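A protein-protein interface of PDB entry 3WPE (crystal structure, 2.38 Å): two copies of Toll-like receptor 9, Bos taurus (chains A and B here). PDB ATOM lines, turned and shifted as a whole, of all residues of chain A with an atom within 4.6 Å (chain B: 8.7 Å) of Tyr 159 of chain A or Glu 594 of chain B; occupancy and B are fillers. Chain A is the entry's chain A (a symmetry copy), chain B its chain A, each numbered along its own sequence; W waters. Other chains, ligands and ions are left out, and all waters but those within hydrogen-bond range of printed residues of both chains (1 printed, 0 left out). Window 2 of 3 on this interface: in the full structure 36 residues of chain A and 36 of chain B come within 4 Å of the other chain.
OE2 of Glu 594 of chain B is in salt-bridge range of NH1 of Arg 241 of chain A. The side-chain sulfur (SD) of Met 160 of chain A lies close to the backbone carbonyl oxygen (O) of Ala 593 of chain B (3.5 Å).
N of Arg 568 of chain B is in hydrogen-bond range of OH of Tyr 598 of chain B, 3.4 Å away. The backbone carbonyl oxygen (O) of Leu 597 of chain B is in hydrogen-bond range of the side-chain amide nitrogen (NE2) of Gln 571 of chain B, 2.9 Å away. The side-chain hydroxyl (OH) of Tyr 159 of chain A lies within hydrogen-bond range of the side-chain amide nitrogen (ND2) of Asn 242 of chain A, 3.4 Å away.
Tyr 159 of chain A touches Glu 594 of chain B (OH to OE1, 3.7 Å). Arg 241 of chain A touches Arg 568 of chain B. O of Arg 241 of chain A touches CD1 of Leu 597 of chain B, 3.7 Å away. Asn 242 of chain A touches Glu 594 of chain B. Asn 242 of chain A touches Leu 597 of chain B (CA to CD1, 3.7 Å). N of Pro 243 of chain A touches CD1 of Leu 597 of chain B (3.9 Å).
Tyr 159 of chain A touches one residue of chain B. Printed residues of chain B within 4 Å of Met 160 of chain A: Ala 593. Printed residues of chain B within 4 Å of Pro 243 of chain A: Leu 597. Printed residues of chain A within 4 Å of Arg 568 of chain B: Arg 241. Of the printed residues of chain A, Leu 597 of chain B touches Arg 241 (3.7 Å), Asn 242 (3.7 Å) and Pro 243 (3.9 Å). The nearest printed residue of chain B that does not touch Asn 242 of chain A is Arg 568 of chain B (6.4 Å).
Of the 9 printed residues of chain A, 5 touch a printed residue of chain B. Printed residues of chain A that touch a printed residue of chain B: Tyr 159, Met 160, Arg 241, Asn 242 and Pro 243. Hydrophobic or aromatic side chains of chain A that line the printed part of chain B: Tyr 159, Met 160 and Pro 243. Along chain A the printed residues that touch a printed residue of chain B span positions 159 to 243. Of the 19 printed residues of chain B, 4 touch a printed residue of chain A. Hydrophobic or aromatic side chains of chain B within 4 Å of the printed part of chain A: Leu 597.
No position is printed for both chains. Of the 8 pairs that touch across the chains among the printed residues, none has its exchanged pair printed and touching as well.
Water W1 lies within hydrogen-bond range of the backbone NH of Arg 568 of chain B (2.7 Å), the backbone carbonyl oxygen of Arg 241 of chain A (2.7 Å) and the side-chain hydroxyl of Tyr 598 of chain B (2.9 Å).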
ATOM      1  N   TYR A 158      28.501  20.959  -0.648  1.00  0.00           N
ATOM      2  CA  TYR A 158      27.983  19.753  -1.286  1.00  0.00           C
ATOM      3  C   TYR A 158      28.524  19.637  -2.704  1.00  0.00           C
ATOM      4  O   TYR A 158      29.288  20.490  -3.154  1.00  0.00           O
ATOM      5  CB  TYR A 158      26.445  19.737  -1.278  1.00  0.00           C
ATOM      6  CG  TYR A 158      25.790  20.651  -2.290  1.00  0.00           C
ATOM      7  CD1 TYR A 158      25.945  22.033  -2.217  1.00  0.00           C
ATOM      8  CD2 TYR A 158      24.980  20.133  -3.300  1.00  0.00           C
ATOM      9  CE1 TYR A 158      25.334  22.863  -3.137  1.00  0.00           C
ATOM     10  CE2 TYR A 158      24.366  20.962  -4.221  1.00  0.00           C
ATOM     11  CZ  TYR A 158      24.544  22.322  -4.130  1.00  0.00           C
ATOM     12  OH  TYR A 158      23.945  23.146  -5.041  1.00  0.00           O
ATOM     13  N   TYR A 159      28.120  18.588  -3.411  1.00  0.00           N
ATOM     14  CA  TYR A 159      28.770  18.227  -4.673  1.00  0.00           C
ATOM     15  C   TYR A 159      28.828  19.366  -5.692  1.00  0.00           C
ATOM     16  O   TYR A 159      29.820  19.497  -6.411  1.00  0.00           O
ATOM     17  CB  TYR A 159      28.134  16.963  -5.283  1.00  0.00           C
ATOM     18  CG  TYR A 159      26.724  17.142  -5.801  1.00  0.00           C
ATOM     19  CD1 TYR A 159      25.623  16.947  -4.973  1.00  0.00           C
ATOM     20  CD2 TYR A 159      26.496  17.487  -7.124  1.00  0.00           C
ATOM     21  CE1 TYR A 159      24.343  17.097  -5.448  1.00  0.00           C
ATOM     22  CE2 TYR A 159      25.215  17.647  -7.603  1.00  0.00           C
ATOM     23  CZ  TYR A 159      24.146  17.449  -6.764  1.00  0.00           C
ATOM     24  OH  TYR A 159      22.882  17.607  -7.254  1.00  0.00           O
ATOM     25  N   MET A 160      27.789  20.196  -5.741  1.00  0.00           N
ATOM     26  CA  MET A 160      27.749  21.312  -6.691  1.00  0.00           C
ATOM     27  C   MET A 160      28.469  22.555  -6.164  1.00  0.00           C
ATOM     28  O   MET A 160      28.719  23.481  -6.923  1.00  0.00           O
ATOM     29  CB  MET A 160      26.302  21.670  -7.042  1.00  0.00           C
ATOM     30  CG  MET A 160      26.107  22.104  -8.482  1.00  0.00           C
ATOM     31  SD  MET A 160      26.324  20.722  -9.614  1.00  0.00           S
ATOM     32  CE  MET A 160      26.698  21.594 -11.131  1.00  0.00           C
ATOM     33  N   ASN A 161      28.778  22.576  -4.869  1.00  0.00           N
ATOM     34  CA  ASN A 161      29.501  23.675  -4.243  1.00  0.00           C
ATOM     35  C   ASN A 161      30.355  23.128  -3.095  1.00  0.00           C
ATOM     36  O   ASN A 161      29.989  23.253  -1.927  1.00  0.00           O
ATOM     37  CB  ASN A 161      28.516  24.728  -3.732  1.00  0.00           C
ATOM     38  CG  ASN A 161      29.202  26.013  -3.309  1.00  0.00           C
ATOM     39  OD1 ASN A 161      30.275  26.358  -3.817  1.00  0.00           O
ATOM     40  ND2 ASN A 161      28.571  26.748  -2.398  1.00  0.00           N
ATOM     41  N   PRO A 162      31.488  22.494  -3.429  1.00  0.00           N
ATOM     42  CA  PRO A 162      32.173  21.670  -2.438  1.00  0.00           C
ATOM     43  C   PRO A 162      33.035  22.433  -1.442  1.00  0.00           C
ATOM     44  O   PRO A 162      33.513  23.530  -1.717  1.00  0.00           O
ATOM     45  CB  PRO A 162      33.034  20.730  -3.292  1.00  0.00           C
ATOM     46  CG  PRO A 162      33.274  21.470  -4.552  1.00  0.00           C
ATOM     47  CD  PRO A 162      32.086  22.368  -4.768  1.00  0.00           C
ATOM     48  N   ARG A 241      19.472  10.155  -8.373  1.00  0.00           N
ATOM     49  CA  ARG A 241      19.841  10.649  -9.704  1.00  0.00           C
ATOM     50  C   ARG A 241      21.088  11.547  -9.680  1.00  0.00           C
ATOM     51  O   ARG A 241      21.580  11.966 -10.724  1.00  0.00           O
ATOM     52  CB  ARG A 241      18.672  11.405 -10.335  1.00  0.00           C
ATOM     53  CG  ARG A 241      18.247  12.677  -9.622  1.00  0.00           C
ATOM     54  CD  ARG A 241      17.314  13.498 -10.495  1.00  0.00           C
ATOM     55  NE  ARG A 241      16.853  14.708  -9.810  1.00  0.00           N
ATOM     56  CZ  ARG A 241      17.378  15.927  -9.953  1.00  0.00           C
ATOM     57  NH1 ARG A 241      18.398  16.149 -10.775  1.00  0.00           N
ATOM     58  NH2 ARG A 241      16.868  16.943  -9.267  1.00  0.00           N
ATOM     59  N   ASN A 242      21.610  11.816  -8.489  1.00  0.00           N
ATOM     60  CA  ASN A 242      22.721  12.735  -8.315  1.00  0.00           C
ATOM     61  C   ASN A 242      23.739  12.104  -7.376  1.00  0.00           C
ATOM     62  O   ASN A 242      23.509  11.000  -6.885  1.00  0.00           O
ATOM     63  CB  ASN A 242      22.198  14.057  -7.752  1.00  0.00           C
ATOM     64  CG  ASN A 242      21.502  13.891  -6.414  1.00  0.00           C
ATOM     65  OD1 ASN A 242      21.252  12.779  -5.957  1.00  0.00           O
ATOM     66  ND2 ASN A 242      21.182  15.008  -5.781  1.00  0.00           N
ATOM     67  N   PRO A 243      24.871  12.791  -7.124  1.00  0.00           N
ATOM     68  CA  PRO A 243      25.840  12.198  -6.213  1.00  0.00           C
ATOM     69  C   PRO A 243      25.232  11.906  -4.841  1.00  0.00           C
ATOM     70  O   PRO A 243      24.455  12.704  -4.318  1.00  0.00           O
ATOM     71  CB  PRO A 243      26.942  13.256  -6.142  1.00  0.00           C
ATOM     72  CG  PRO A 243      26.874  13.920  -7.475  1.00  0.00           C
ATOM     73  CD  PRO A 243      25.406  14.005  -7.766  1.00  0.00           C
ATOM     74  N   ARG A 245      25.830   9.327  -1.080  1.00  0.00           N
ATOM     75  CA  ARG A 245      26.627   8.445  -0.240  1.00  0.00           C
ATOM     76  C   ARG A 245      25.630   7.597   0.521  1.00  0.00           C
ATOM     77  O   ARG A 245      24.793   8.125   1.252  1.00  0.00           O
ATOM     78  CB  ARG A 245      27.537   9.201   0.740  1.00  0.00           C
ATOM     79  CG  ARG A 245      27.686  10.700   0.525  1.00  0.00           C
ATOM     80  CD  ARG A 245      28.640  11.084  -0.595  1.00  0.00           C
ATOM     81  NE  ARG A 245      28.654  12.544  -0.749  1.00  0.00           N
ATOM     82  CZ  ARG A 245      28.504  13.210  -1.896  1.00  0.00           C
ATOM     83  NH1 ARG A 245      28.365  12.569  -3.050  1.00  0.00           N
ATOM     84  NH2 ARG A 245      28.522  14.542  -1.891  1.00  0.00           N
ATOM     85  N   GLN B 540       9.807   9.424 -14.786  1.00  0.00           N
ATOM     86  CA  GLN B 540      10.547  10.044 -13.700  1.00  0.00           C
ATOM     87  C   GLN B 540      10.737   9.026 -12.582  1.00  0.00           C
ATOM     88  O   GLN B 540       9.845   8.223 -12.314  1.00  0.00           O
ATOM     89  CB  GLN B 540       9.793  11.265 -13.169  1.00  0.00           C
ATOM     90  CG  GLN B 540      10.673  12.271 -12.445  1.00  0.00           C
ATOM     91  CD  GLN B 540      11.508  13.102 -13.400  1.00  0.00           C
ATOM     92  OE1 GLN B 540      12.725  12.921 -13.499  1.00  0.00           O
ATOM     93  NE2 GLN B 540      10.858  14.014 -14.114  1.00  0.00           N
ATOM     94  N   HIS B 566      17.333  11.911 -19.679  1.00  0.00           N
ATOM     95  CA  HIS B 566      17.718  13.075 -18.866  1.00  0.00           C
ATOM     96  C   HIS B 566      18.347  12.757 -17.504  1.00  0.00           C
ATOM     97  O   HIS B 566      19.138  13.556 -16.999  1.00  0.00           O
ATOM     98  CB  HIS B 566      16.525  14.032 -18.684  1.00  0.00           C
ATOM     99  CG  HIS B 566      15.425  13.486 -17.831  1.00  0.00           C
ATOM    100  ND1 HIS B 566      14.375  12.758 -18.350  1.00  0.00           N
ATOM    101  CD2 HIS B 566      15.207  13.566 -16.499  1.00  0.00           C
ATOM    102  CE1 HIS B 566      13.559  12.411 -17.372  1.00  0.00           C
ATOM    103  NE2 HIS B 566      14.042  12.887 -16.238  1.00  0.00           N
ATOM    104  N   SER B 567      17.989  11.622 -16.900  1.00  0.00           N
ATOM    105  CA  SER B 567      18.597  11.207 -15.631  1.00  0.00           C
ATOM    106  C   SER B 567      18.401   9.709 -15.338  1.00  0.00           C
ATOM    107  O   SER B 567      17.737   8.992 -16.094  1.00  0.00           O
ATOM    108  CB  SER B 567      18.036  12.057 -14.480  1.00  0.00           C
ATOM    109  OG  SER B 567      16.660  11.816 -14.294  1.00  0.00           O
ATOM    110  N   ARG B 568      18.997   9.252 -14.237  1.00  0.00           N
ATOM    111  CA  ARG B 568      18.964   7.841 -13.821  1.00  0.00           C
ATOM    112  C   ARG B 568      19.296   6.883 -14.963  1.00  0.00           C
ATOM    113  O   ARG B 568      18.633   5.864 -15.170  1.00  0.00           O
ATOM    114  CB  ARG B 568      17.621   7.495 -13.172  1.00  0.00           C
ATOM    115  CG  ARG B 568      17.454   8.113 -11.796  1.00  0.00           C
ATOM    116  CD  ARG B 568      16.161   7.682 -11.129  1.00  0.00           C
ATOM    117  NE  ARG B 568      16.022   8.322  -9.824  1.00  0.00           N
ATOM    118  CZ  ARG B 568      15.479   9.520  -9.606  1.00  0.00           C
ATOM    119  NH1 ARG B 568      14.984  10.250 -10.600  1.00  0.00           N
ATOM    120  NH2 ARG B 568      15.428   9.992  -8.368  1.00  0.00           N
ATOM    121  N   GLN B 571      26.059   5.560 -16.580  1.00  0.00           N
ATOM    122  CA  GLN B 571      27.007   6.671 -16.568  1.00  0.00           C
ATOM    123  C   GLN B 571      27.968   6.639 -17.756  1.00  0.00           C
ATOM    124  O   GLN B 571      28.501   7.683 -18.153  1.00  0.00           O
ATOM    125  CB  GLN B 571      27.777   6.706 -15.244  1.00  0.00           C
ATOM    126  CG  GLN B 571      26.881   6.962 -14.044  1.00  0.00           C
ATOM    127  CD  GLN B 571      27.642   7.108 -12.744  1.00  0.00           C
ATOM    128  OE1 GLN B 571      27.418   6.358 -11.798  1.00  0.00           O
ATOM    129  NE2 GLN B 571      28.534   8.084 -12.684  1.00  0.00           N
ATOM    130  N   SER B 587      18.084  15.108 -23.161  1.00  0.00           N
ATOM    131  CA  SER B 587      18.475  16.192 -22.254  1.00  0.00           C
ATOM    132  C   SER B 587      19.857  15.919 -21.673  1.00  0.00           C
ATOM    133  O   SER B 587      20.030  15.741 -20.466  1.00  0.00           O
ATOM    134  CB  SER B 587      17.447  16.371 -21.137  1.00  0.00           C
ATOM    135  OG  SER B 587      16.129  16.431 -21.666  1.00  0.00           O
ATOM    136  N   LEU B 588      20.845  15.882 -22.552  1.00  0.00           N
ATOM    137  CA  LEU B 588      22.233  15.821 -22.123  1.00  0.00           C
ATOM    138  C   LEU B 588      22.589  17.014 -21.226  1.00  0.00           C
ATOM    139  O   LEU B 588      23.441  16.895 -20.358  1.00  0.00           O
ATOM    140  CB  LEU B 588      23.166  15.758 -23.335  1.00  0.00           C
ATOM    141  CG  LEU B 588      24.653  15.526 -23.050  1.00  0.00           C
ATOM    142  CD1 LEU B 588      24.889  14.300 -22.187  1.00  0.00           C
ATOM    143  CD2 LEU B 588      25.404  15.391 -24.364  1.00  0.00           C
ATOM    144  N   SER B 589      21.927  18.155 -21.430  1.00  0.00           N
ATOM    145  CA  SER B 589      22.104  19.331 -20.568  1.00  0.00           C
ATOM    146  C   SER B 589      21.873  19.012 -19.102  1.00  0.00           C
ATOM    147  O   SER B 589      22.724  19.287 -18.261  1.00  0.00           O
ATOM    148  CB  SER B 589      21.148  20.448 -20.977  1.00  0.00           C
ATOM    149  OG  SER B 589      21.435  21.632 -20.252  1.00  0.00           O
ATOM    150  N   GLN B 590      20.717  18.432 -18.800  1.00  0.00           N
ATOM    151  CA  GLN B 590      20.380  18.065 -17.427  1.00  0.00           C
ATOM    152  C   GLN B 590      21.308  16.972 -16.868  1.00  0.00           C
ATOM    153  O   GLN B 590      21.625  16.972 -15.678  1.00  0.00           O
ATOM    154  CB  GLN B 590      18.924  17.611 -17.341  1.00  0.00           C
ATOM    155  CG  GLN B 590      18.341  17.686 -15.942  1.00  0.00           C
ATOM    156  CD  GLN B 590      17.025  16.943 -15.821  1.00  0.00           C
ATOM    157  OE1 GLN B 590      16.180  16.997 -16.721  1.00  0.00           O
ATOM    158  NE2 GLN B 590      16.839  16.245 -14.700  1.00  0.00           N
ATOM    159  N   MET B 591      21.738  16.054 -17.732  1.00  0.00           N
ATOM    160  CA  MET B 591      22.683  15.007 -17.352  1.00  0.00           C
ATOM    161  C   MET B 591      24.023  15.610 -16.962  1.00  0.00           C
ATOM    162  O   MET B 591      24.667  15.157 -16.021  1.00  0.00           O
ATOM    163  CB  MET B 591      22.904  14.032 -18.507  1.00  0.00           C
ATOM    164  CG  MET B 591      21.705  13.168 -18.828  1.00  0.00           C
ATOM    165  SD  MET B 591      21.899  12.327 -20.406  1.00  0.00           S
ATOM    166  CE  MET B 591      23.263  11.217 -20.049  1.00  0.00           C
ATOM    167  N   TRP B 592      24.437  16.635 -17.694  1.00  0.00           N
ATOM    168  CA  TRP B 592      25.695  17.298 -17.418  1.00  0.00           C
ATOM    169  C   TRP B 592      25.578  18.389 -16.359  1.00  0.00           C
ATOM    170  O   TRP B 592      26.566  19.032 -16.048  1.00  0.00           O
ATOM    171  CB  TRP B 592      26.299  17.858 -18.707  1.00  0.00           C
ATOM    172  CG  TRP B 592      27.010  16.833 -19.553  1.00  0.00           C
ATOM    173  CD1 TRP B 592      27.396  15.565 -19.190  1.00  0.00           C
ATOM    174  CD2 TRP B 592      27.476  17.021 -20.889  1.00  0.00           C
ATOM    175  NE1 TRP B 592      28.035  14.949 -20.237  1.00  0.00           N
ATOM    176  CE2 TRP B 592      28.099  15.823 -21.290  1.00  0.00           C
ATOM    177  CE3 TRP B 592      27.412  18.084 -21.795  1.00  0.00           C
ATOM    178  CZ2 TRP B 592      28.652  15.661 -22.550  1.00  0.00           C
ATOM    179  CZ3 TRP B 592      27.965  17.920 -23.047  1.00  0.00           C
ATOM    180  CH2 TRP B 592      28.577  16.715 -23.413  1.00  0.00           C
ATOM    181  N   ALA B 593      24.383  18.596 -15.808  1.00  0.00           N
ATOM    182  CA  ALA B 593      24.219  19.426 -14.614  1.00  0.00           C
ATOM    183  C   ALA B 593      24.447  18.609 -13.338  1.00  0.00           C
ATOM    184  O   ALA B 593      24.788  19.170 -12.296  1.00  0.00           O
ATOM    185  CB  ALA B 593      22.838  20.051 -14.583  1.00  0.00           C
ATOM    186  N   GLU B 594      24.262  17.292 -13.425  1.00  0.00           N
ATOM    187  CA  GLU B 594      24.358  16.403 -12.259  1.00  0.00           C
ATOM    188  C   GLU B 594      25.804  16.073 -11.860  1.00  0.00           C
ATOM    189  O   GLU B 594      26.222  14.914 -11.897  1.00  0.00           O
ATOM    190  CB  GLU B 594      23.583  15.105 -12.527  1.00  0.00           C
ATOM    191  CG  GLU B 594      22.081  15.292 -12.638  1.00  0.00           C
ATOM    192  CD  GLU B 594      21.418  15.480 -11.287  1.00  0.00           C
ATOM    193  OE1 GLU B 594      21.776  16.426 -10.558  1.00  0.00           O
ATOM    194  OE2 GLU B 594      20.517  14.685 -10.957  1.00  0.00           O
ATOM    195  N   GLY B 595      26.554  17.096 -11.463  1.00  0.00           N
ATOM    196  CA  GLY B 595      27.958  16.928 -11.102  1.00  0.00           C
ATOM    197  C   GLY B 595      28.750  16.360 -12.257  1.00  0.00           C
ATOM    198  O   GLY B 595      28.478  16.672 -13.416  1.00  0.00           O
ATOM    199  N   ASP B 596      29.719  15.508 -11.946  1.00  0.00           N
ATOM    200  CA  ASP B 596      30.535  14.867 -12.976  1.00  0.00           C
ATOM    201  C   ASP B 596      30.110  13.420 -13.229  1.00  0.00           C
ATOM    202  O   ASP B 596      30.804  12.690 -13.918  1.00  0.00           O
ATOM    203  CB  ASP B 596      32.028  14.964 -12.621  1.00  0.00           C
ATOM    204  CG  ASP B 596      32.413  14.098 -11.436  1.00  0.00           C
ATOM    205  OD1 ASP B 596      31.512  13.670 -10.676  1.00  0.00           O
ATOM    206  OD2 ASP B 596      33.628  13.850 -11.266  1.00  0.00           O
ATOM    207  N   LEU B 597      28.956  13.021 -12.695  1.00  0.00           N
ATOM    208  CA  LEU B 597      28.393  11.687 -12.941  1.00  0.00           C
ATOM    209  C   LEU B 597      28.379  11.286 -14.412  1.00  0.00           C
ATOM    210  O   LEU B 597      28.578  10.118 -14.730  1.00  0.00           O
ATOM    211  CB  LEU B 597      26.956  11.585 -12.415  1.00  0.00           C
ATOM    212  CG  LEU B 597      26.670  11.661 -10.914  1.00  0.00           C
ATOM    213  CD1 LEU B 597      25.197  11.379 -10.694  1.00  0.00           C
ATOM    214  CD2 LEU B 597      27.511  10.695 -10.087  1.00  0.00           C
ATOM    215  N   TYR B 598      28.139  12.237 -15.304  1.00  0.00           N
ATOM    216  CA  TYR B 598      28.016  11.926 -16.734  1.00  0.00           C
ATOM    217  C   TYR B 598      29.091  12.586 -17.598  1.00  0.00           C
ATOM    218  O   TYR B 598      28.889  12.783 -18.797  1.00  0.00           O
ATOM    219  CB  TYR B 598      26.630  12.340 -17.244  1.00  0.00           C
ATOM    220  CG  TYR B 598      25.495  11.582 -16.601  1.00  0.00           C
ATOM    221  CD1 TYR B 598      25.146  10.313 -17.038  1.00  0.00           C
ATOM    222  CD2 TYR B 598      24.779  12.132 -15.552  1.00  0.00           C
ATOM    223  CE1 TYR B 598      24.106   9.617 -16.450  1.00  0.00           C
ATOM    224  CE2 TYR B 598      23.735  11.448 -14.963  1.00  0.00           C
ATOM    225  CZ  TYR B 598      23.397  10.193 -15.416  1.00  0.00           C
ATOM    226  OH  TYR B 598      22.353   9.524 -14.815  1.00  0.00           O
ATOM    227  N   LEU B 599      30.235  12.902 -16.995  1.00  0.00           N
ATOM    228  CA  LEU B 599      31.327  13.564 -17.706  1.00  0.00           C
ATOM    229  C   LEU B 599      31.923  12.665 -18.795  1.00  0.00           C
ATOM    230  O   LEU B 599      32.363  13.150 -19.839  1.00  0.00           O
ATOM    231  CB  LEU B 599      32.433  13.971 -16.725  1.00  0.00           C
ATOM    232  CG  LEU B 599      33.103  15.314 -17.018  1.00  0.00           C
ATOM    233  CD1 LEU B 599      32.332  16.426 -16.315  1.00  0.00           C
ATOM    234  CD2 LEU B 599      34.563  15.314 -16.583  1.00  0.00           C
ATOM    235  N   HIS B 625      33.818  18.700 -21.356  1.00  0.00           N
ATOM    236  CA  HIS B 625      32.946  17.735 -22.020  1.00  0.00           C
ATOM    237  C   HIS B 625      33.585  17.269 -23.312  1.00  0.00           C
ATOM    238  O   HIS B 625      33.661  16.071 -23.582  1.00  0.00           O
ATOM    239  CB  HIS B 625      31.565  18.330 -22.315  1.00  0.00           C
ATOM    240  CG  HIS B 625      30.844  18.826 -21.102  1.00  0.00           C
ATOM    241  ND1 HIS B 625      30.280  20.081 -21.038  1.00  0.00           N
ATOM    242  CD2 HIS B 625      30.604  18.243 -19.902  1.00  0.00           C
ATOM    243  CE1 HIS B 625      29.718  20.249 -19.856  1.00  0.00           C
ATOM    244  NE2 HIS B 625      29.898  19.148 -19.148  1.00  0.00           N
HETATM  245  O   HOH W   1      20.600  11.078 -13.115  1.00  0.00           O
